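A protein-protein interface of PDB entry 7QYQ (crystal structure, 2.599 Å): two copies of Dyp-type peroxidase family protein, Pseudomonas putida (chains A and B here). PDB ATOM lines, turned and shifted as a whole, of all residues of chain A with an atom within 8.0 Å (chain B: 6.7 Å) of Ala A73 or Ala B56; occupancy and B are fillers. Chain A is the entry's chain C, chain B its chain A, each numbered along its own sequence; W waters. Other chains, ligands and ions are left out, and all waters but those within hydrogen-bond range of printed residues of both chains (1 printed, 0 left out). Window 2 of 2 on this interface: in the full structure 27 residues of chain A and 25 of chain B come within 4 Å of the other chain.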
ATOM      1  N   LEU A  70      -1.109  -4.416   2.840  1.00  0.00           N
ATOM      2  CA  LEU A  70      -2.513  -4.732   3.082  1.00  0.00           C
ATOM      3  C   LEU A  70      -2.824  -4.518   4.559  1.00  0.00           C
ATOM      4  O   LEU A  70      -2.341  -5.264   5.417  1.00  0.00           O
ATOM      5  CB  LEU A  70      -2.830  -6.166   2.661  1.00  0.00           C
ATOM      6  CG  LEU A  70      -3.246  -6.417   1.209  1.00  0.00           C
ATOM      7  CD1 LEU A  70      -2.126  -6.079   0.233  1.00  0.00           C
ATOM      8  CD2 LEU A  70      -3.706  -7.857   1.024  1.00  0.00           C
ATOM      9  N   ASP A  71      -3.633  -3.499   4.852  1.00  0.00           N
ATOM     10  CA  ASP A  71      -4.095  -3.232   6.214  1.00  0.00           C
ATOM     11  C   ASP A  71      -5.319  -4.104   6.479  1.00  0.00           C
ATOM     12  O   ASP A  71      -6.470  -3.666   6.407  1.00  0.00           O
ATOM     13  CB  ASP A  71      -4.400  -1.752   6.401  1.00  0.00           C
ATOM     14  CG  ASP A  71      -4.682  -1.390   7.848  1.00  0.00           C
ATOM     15  OD1 ASP A  71      -4.526  -2.263   8.727  1.00  0.00           O
ATOM     16  OD2 ASP A  71      -5.060  -0.227   8.105  1.00  0.00           O
ATOM     17  N   ALA A  72      -5.059  -5.371   6.790  1.00  0.00           N
ATOM     18  CA  ALA A  72      -6.102  -6.363   7.010  1.00  0.00           C
ATOM     19  C   ALA A  72      -5.903  -7.008   8.377  1.00  0.00           C
ATOM     20  O   ALA A  72      -4.959  -6.691   9.107  1.00  0.00           O
ATOM     21  CB  ALA A  72      -6.105  -7.421   5.901  1.00  0.00           C
ATOM     22  N   ALA A  73      -6.808  -7.922   8.725  1.00  0.00           N
ATOM     23  CA  ALA A  73      -6.712  -8.637   9.991  1.00  0.00           C
ATOM     24  C   ALA A  73      -5.726  -9.795   9.947  1.00  0.00           C
ATOM     25  O   ALA A  73      -5.446 -10.388  10.996  1.00  0.00           O
ATOM     26  CB  ALA A  73      -8.090  -9.154  10.411  1.00  0.00           C
ATOM     27  N   VAL A  74      -5.196 -10.130   8.773  1.00  0.00           N
ATOM     28  CA  VAL A  74      -4.165 -11.148   8.640  1.00  0.00           C
ATOM     29  C   VAL A  74      -2.891 -10.476   8.149  1.00  0.00           C
ATOM     30  O   VAL A  74      -2.903  -9.344   7.656  1.00  0.00           O
ATOM     31  CB  VAL A  74      -4.585 -12.293   7.696  1.00  0.00           C
ATOM     32  CG1 VAL A  74      -5.709 -13.105   8.321  1.00  0.00           C
ATOM     33  CG2 VAL A  74      -5.008 -11.739   6.347  1.00  0.00           C
ATOM     34  N   GLU A  75      -1.779 -11.191   8.287  1.00  0.00           N
ATOM     35  CA  GLU A  75      -0.457 -10.639   8.023  1.00  0.00           C
ATOM     36  C   GLU A  75       0.071 -11.157   6.690  1.00  0.00           C
ATOM     37  O   GLU A  75       0.290 -12.362   6.528  1.00  0.00           O
ATOM     38  CB  GLU A  75       0.508 -10.986   9.155  1.00  0.00           C
ATOM     39  CG  GLU A  75       0.143 -10.352  10.488  1.00  0.00           C
ATOM     40  CD  GLU A  75       0.946 -10.916  11.641  1.00  0.00           C
ATOM     41  OE1 GLU A  75       2.022 -11.497  11.387  1.00  0.00           O
ATOM     42  OE2 GLU A  75       0.505 -10.776  12.801  1.00  0.00           O
ATOM     43  N   ASN A  76       0.273 -10.241   5.743  1.00  0.00           N
ATOM     44  CA  ASN A  76       0.933 -10.520   4.469  1.00  0.00           C
ATOM     45  C   ASN A  76       2.146  -9.601   4.390  1.00  0.00           C
ATOM     46  O   ASN A  76       2.045  -8.468   3.891  1.00  0.00           O
ATOM     47  CB  ASN A  76      -0.011 -10.303   3.287  1.00  0.00           C
ATOM     48  CG  ASN A  76      -1.166 -11.290   3.270  1.00  0.00           C
ATOM     49  OD1 ASN A  76      -0.992 -12.461   2.936  1.00  0.00           O
ATOM     50  ND2 ASN A  76      -2.356 -10.817   3.626  1.00  0.00           N
ATOM     51  N   SER A 247      -7.767 -11.683   2.229  1.00  0.00           N
ATOM     52  CA  SER A 247      -7.489 -10.998   3.485  1.00  0.00           C
ATOM     53  C   SER A 247      -8.720 -10.337   4.091  1.00  0.00           C
ATOM     54  O   SER A 247      -8.600  -9.678   5.129  1.00  0.00           O
ATOM     55  CB  SER A 247      -6.393  -9.950   3.277  1.00  0.00           C
ATOM     56  OG  SER A 247      -5.217 -10.538   2.751  1.00  0.00           O
ATOM     57  N   GLY A 248      -9.892 -10.496   3.480  1.00  0.00           N
ATOM     58  CA  GLY A 248     -11.102  -9.904   4.007  1.00  0.00           C
ATOM     59  C   GLY A 248     -11.265  -8.425   3.742  1.00  0.00           C
ATOM     60  O   GLY A 248     -12.119  -7.791   4.371  1.00  0.00           O
ATOM     61  N   LEU A 249     -10.473  -7.852   2.835  1.00  0.00           N
ATOM     62  CA  LEU A 249     -10.556  -6.429   2.537  1.00  0.00           C
ATOM     63  C   LEU A 249     -11.681  -6.082   1.571  1.00  0.00           C
ATOM     64  O   LEU A 249     -11.963  -4.894   1.379  1.00  0.00           O
ATOM     65  CB  LEU A 249      -9.224  -5.931   1.970  1.00  0.00           C
ATOM     66  CG  LEU A 249      -8.037  -5.937   2.934  1.00  0.00           C
ATOM     67  CD1 LEU A 249      -6.788  -5.393   2.259  1.00  0.00           C
ATOM     68  CD2 LEU A 249      -8.374  -5.124   4.168  1.00  0.00           C
ATOM     69  N   GLY A 252     -15.052  -8.742   3.976  1.00  0.00           N
ATOM     70  CA  GLY A 252     -14.899  -9.043   5.383  1.00  0.00           C
ATOM     71  C   GLY A 252     -14.694 -10.505   5.714  1.00  0.00           C
ATOM     72  O   GLY A 252     -14.505 -10.834   6.892  1.00  0.00           O
ATOM     73  N   ILE A 254     -12.410 -13.809   5.564  1.00  0.00           N
ATOM     74  CA  ILE A 254     -10.989 -14.124   5.459  1.00  0.00           C
ATOM     75  C   ILE A 254     -10.826 -15.557   4.972  1.00  0.00           C
ATOM     76  O   ILE A 254     -11.588 -16.452   5.365  1.00  0.00           O
ATOM     77  CB  ILE A 254     -10.282 -13.903   6.811  1.00  0.00           C
ATOM     78  CG1 ILE A 254     -10.275 -12.413   7.162  1.00  0.00           C
ATOM     79  CG2 ILE A 254      -8.861 -14.454   6.787  1.00  0.00           C
ATOM     80  CD1 ILE A 254      -9.585 -12.088   8.468  1.00  0.00           C
ATOM     81  N   TYR A 258      -5.499 -19.075   6.330  1.00  0.00           N
ATOM     82  CA  TYR A 258      -4.851 -18.432   7.467  1.00  0.00           C
ATOM     83  C   TYR A 258      -5.106 -19.146   8.789  1.00  0.00           C
ATOM     84  O   TYR A 258      -4.519 -18.752   9.802  1.00  0.00           O
ATOM     85  CB  TYR A 258      -5.305 -16.974   7.567  1.00  0.00           C
ATOM     86  CG  TYR A 258      -4.844 -16.116   6.411  1.00  0.00           C
ATOM     87  CD1 TYR A 258      -3.553 -15.600   6.374  1.00  0.00           C
ATOM     88  CD2 TYR A 258      -5.693 -15.829   5.350  1.00  0.00           C
ATOM     89  CE1 TYR A 258      -3.125 -14.818   5.316  1.00  0.00           C
ATOM     90  CE2 TYR A 258      -5.273 -15.049   4.288  1.00  0.00           C
ATOM     91  CZ  TYR A 258      -3.989 -14.546   4.276  1.00  0.00           C
ATOM     92  OH  TYR A 258      -3.569 -13.769   3.221  1.00  0.00           O
ATOM     93  N   LEU B  23      -1.822 -12.906  15.437  1.00  0.00           N
ATOM     94  CA  LEU B  23      -3.146 -13.320  15.898  1.00  0.00           C
ATOM     95  C   LEU B  23      -3.586 -14.505  15.051  1.00  0.00           C
ATOM     96  O   LEU B  23      -4.160 -14.355  13.972  1.00  0.00           O
ATOM     97  CB  LEU B  23      -4.136 -12.167  15.816  1.00  0.00           C
ATOM     98  CG  LEU B  23      -5.491 -12.439  16.473  1.00  0.00           C
ATOM     99  CD1 LEU B  23      -5.343 -12.565  17.982  1.00  0.00           C
ATOM    100  CD2 LEU B  23      -6.475 -11.342  16.127  1.00  0.00           C
ATOM    101  N   PRO B  26      -8.317 -15.586  16.639  1.00  0.00           N
ATOM    102  CA  PRO B  26      -8.926 -14.392  17.251  1.00  0.00           C
ATOM    103  C   PRO B  26     -10.050 -14.697  18.225  1.00  0.00           C
ATOM    104  O   PRO B  26     -10.331 -13.856  19.088  1.00  0.00           O
ATOM    105  CB  PRO B  26      -9.447 -13.602  16.039  1.00  0.00           C
ATOM    106  CG  PRO B  26      -8.730 -14.175  14.851  1.00  0.00           C
ATOM    107  CD  PRO B  26      -8.494 -15.617  15.179  1.00  0.00           C
ATOM    108  N   LEU B  29      -8.950 -14.869  22.012  1.00  0.00           N
ATOM    109  CA  LEU B  29      -8.322 -13.633  22.464  1.00  0.00           C
ATOM    110  C   LEU B  29      -8.714 -13.241  23.889  1.00  0.00           C
ATOM    111  O   LEU B  29      -7.843 -12.797  24.648  1.00  0.00           O
ATOM    112  CB  LEU B  29      -8.667 -12.492  21.501  1.00  0.00           C
ATOM    113  CG  LEU B  29      -7.905 -11.183  21.717  1.00  0.00           C
ATOM    114  CD1 LEU B  29      -6.408 -11.449  21.737  1.00  0.00           C
ATOM    115  CD2 LEU B  29      -8.253 -10.155  20.648  1.00  0.00           C
ATOM    116  N   ALA B  51      -1.607  -2.841  13.975  1.00  0.00           N
ATOM    117  CA  ALA B  51      -2.781  -2.655  13.126  1.00  0.00           C
ATOM    118  C   ALA B  51      -3.588  -3.930  12.889  1.00  0.00           C
ATOM    119  O   ALA B  51      -4.828  -3.835  12.855  1.00  0.00           O
ATOM    120  CB  ALA B  51      -2.356  -2.032  11.790  1.00  0.00           C
ATOM    121  N   PRO B  52      -2.991  -5.117  12.706  1.00  0.00           N
ATOM    122  CA  PRO B  52      -3.832  -6.316  12.538  1.00  0.00           C
ATOM    123  C   PRO B  52      -4.744  -6.595  13.721  1.00  0.00           C
ATOM    124  O   PRO B  52      -5.877  -7.053  13.526  1.00  0.00           O
ATOM    125  CB  PRO B  52      -2.802  -7.437  12.336  1.00  0.00           C
ATOM    126  CG  PRO B  52      -1.618  -6.753  11.765  1.00  0.00           C
ATOM    127  CD  PRO B  52      -1.570  -5.414  12.435  1.00  0.00           C
ATOM    128  N   LEU B  53      -4.284  -6.329  14.946  1.00  0.00           N
ATOM    129  CA  LEU B  53      -5.122  -6.570  16.118  1.00  0.00           C
ATOM    130  C   LEU B  53      -6.316  -5.623  16.154  1.00  0.00           C
ATOM    131  O   LEU B  53      -7.432  -6.036  16.490  1.00  0.00           O
ATOM    132  CB  LEU B  53      -4.293  -6.435  17.395  1.00  0.00           C
ATOM    133  CG  LEU B  53      -5.022  -6.736  18.706  1.00  0.00           C
ATOM    134  CD1 LEU B  53      -5.608  -8.138  18.685  1.00  0.00           C
ATOM    135  CD2 LEU B  53      -4.087  -6.563  19.893  1.00  0.00           C
ATOM    136  N   ALA B  54      -6.099  -4.348  15.820  1.00  0.00           N
ATOM    137  CA  ALA B  54      -7.206  -3.400  15.781  1.00  0.00           C
ATOM    138  C   ALA B  54      -8.191  -3.744  14.672  1.00  0.00           C
ATOM    139  O   ALA B  54      -9.408  -3.615  14.851  1.00  0.00           O
ATOM    140  CB  ALA B  54      -6.673  -1.978  15.608  1.00  0.00           C
ATOM    141  N   LYS B  55      -7.685  -4.187  13.519  1.00  0.00           N
ATOM    142  CA  LYS B  55      -8.570  -4.537  12.412  1.00  0.00           C
ATOM    143  C   LYS B  55      -9.359  -5.808  12.704  1.00  0.00           C
ATOM    144  O   LYS B  55     -10.517  -5.926  12.285  1.00  0.00           O
ATOM    145  CB  LYS B  55      -7.761  -4.694  11.125  1.00  0.00           C
ATOM    146  CG  LYS B  55      -8.606  -5.006   9.902  1.00  0.00           C
ATOM    147  CD  LYS B  55      -9.506  -3.826   9.568  1.00  0.00           C
ATOM    148  CE  LYS B  55     -10.358  -4.097   8.341  1.00  0.00           C
ATOM    149  NZ  LYS B  55      -9.521  -4.294   7.129  1.00  0.00           N
ATOM    150  N   ALA B  56      -8.754  -6.764  13.414  1.00  0.00           N
ATOM    151  CA  ALA B  56      -9.440  -8.017  13.707  1.00  0.00           C
ATOM    152  C   ALA B  56     -10.608  -7.820  14.664  1.00  0.00           C
ATOM    153  O   ALA B  56     -11.627  -8.509  14.544  1.00  0.00           O
ATOM    154  CB  ALA B  56      -8.452  -9.031  14.280  1.00  0.00           C
ATOM    155  N   LEU B  57     -10.485  -6.897  15.615  1.00  0.00           N
ATOM    156  CA  LEU B  57     -11.559  -6.602  16.553  1.00  0.00           C
ATOM    157  C   LEU B  57     -12.518  -5.538  16.041  1.00  0.00           C
ATOM    158  O   LEU B  57     -13.425  -5.135  16.778  1.00  0.00           O
ATOM    159  CB  LEU B  57     -10.985  -6.165  17.904  1.00  0.00           C
ATOM    160  CG  LEU B  57     -10.187  -7.215  18.676  1.00  0.00           C
ATOM    161  CD1 LEU B  57      -9.618  -6.613  19.948  1.00  0.00           C
ATOM    162  CD2 LEU B  57     -11.065  -8.415  18.992  1.00  0.00           C
ATOM    163  N   GLY B  58     -12.344  -5.078  14.804  1.00  0.00           N
ATOM    164  CA  GLY B  58     -13.221  -4.058  14.255  1.00  0.00           C
ATOM    165  C   GLY B  58     -13.140  -2.723  14.959  1.00  0.00           C
ATOM    166  O   GLY B  58     -14.148  -2.015  15.049  1.00  0.00           O
ATOM    167  N   ARG B  59     -11.964  -2.359  15.463  1.00  0.00           N
ATOM    168  CA  ARG B  59     -11.756  -1.089  16.139  1.00  0.00           C
ATOM    169  C   ARG B  59     -10.716  -0.269  15.388  1.00  0.00           C
ATOM    170  O   ARG B  59      -9.771  -0.814  14.809  1.00  0.00           O
ATOM    171  CB  ARG B  59     -11.299  -1.291  17.589  1.00  0.00           C
ATOM    172  CG  ARG B  59     -12.329  -1.952  18.489  1.00  0.00           C
ATOM    173  CD  ARG B  59     -13.514  -1.033  18.735  1.00  0.00           C
ATOM    174  NE  ARG B  59     -14.519  -1.649  19.596  1.00  0.00           N
ATOM    175  CZ  ARG B  59     -14.556  -1.507  20.917  1.00  0.00           C
ATOM    176  NH1 ARG B  59     -13.643  -0.769  21.533  1.00  0.00           N
ATOM    177  NH2 ARG B  59     -15.508  -2.101  21.624  1.00  0.00           N
ATOM    178  N   ALA B  82       0.586  -8.365  15.125  1.00  0.00           N
ATOM    179  CA  ALA B  82      -0.589  -7.936  15.877  1.00  0.00           C
ATOM    180  C   ALA B  82      -0.217  -7.337  17.229  1.00  0.00           C
ATOM    181  O   ALA B  82      -0.823  -6.349  17.659  1.00  0.00           O
ATOM    182  CB  ALA B  82      -1.547  -9.111  16.068  1.00  0.00           C
HETATM  183  O   HOH W   1      -2.419 -10.587  13.124  1.00  0.00           O
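Of the printed residues of chain B, Asp A71 touches Ala B51 (3.8 Å) and Lys B55 (3.2 Å). Of the printed residues of chain B, Glu A75 touches Ala B82 (3.3 Å). Of the printed residues of chain B, Leu A249 touches Lys B55. Printed residues of chain A within 4 Å of Pro B52: Ala A72 (3.6 Å) and Ala A73 (3.96 Å). Of chain A, only Ala A73 comes within 4 Å of Ala B56. Leu B57 touches none of the printed residues of chain A. Of the printed residues of chain A, Ala B82 touches Glu A75 (3.3 Å). The nearest residue of chain B that does not touch Ala A73 is Leu B23 (5.1 Å). The nearest printed residue of chain A that does not touch Pro B52 is Glu A75 (4.2 Å).
No position is printed for both chains.
Water W1 bridges the side-chain carboxylate (OE2) of Glu A75 and the backbone NH (N) of Leu B23.
Hydrophobic or aromatic side chains of chain A within 4 Å of the printed part of chain B: Ala A73 and Leu A249. Of the 13 printed residues of chain B, 5 touch a printed residue of chain A. Among the printed residues, no Asp or Glu carboxylate lies within 4 Å of a Lys or Arg side-chain nitrogen of the other chain.
OD1 of Asp A71 touches CB of Ala B51, 3.8 Å away. Ala A72 touches Pro B52. Ala A72 touches Lys B55 (C to CG, 3.7 Å). Ala A73 touches Pro B52. N of Ala A73 touches CG of Lys B55, at 3.6 Å. CB of Ala A73 touches CA of Ala B56, at 3.7 Å. CD2 of Leu A249 touches NZ of Lys B55, at 3.3 Å.
The side-chain amino group (NZ) of Lys B55 sits at hydrogen-bond distance from the backbone carbonyl oxygen (O) of Asp A71, at 3.2 Å. OE2 of Glu A75 lies within hydrogen-bond range of N of Ala B82.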
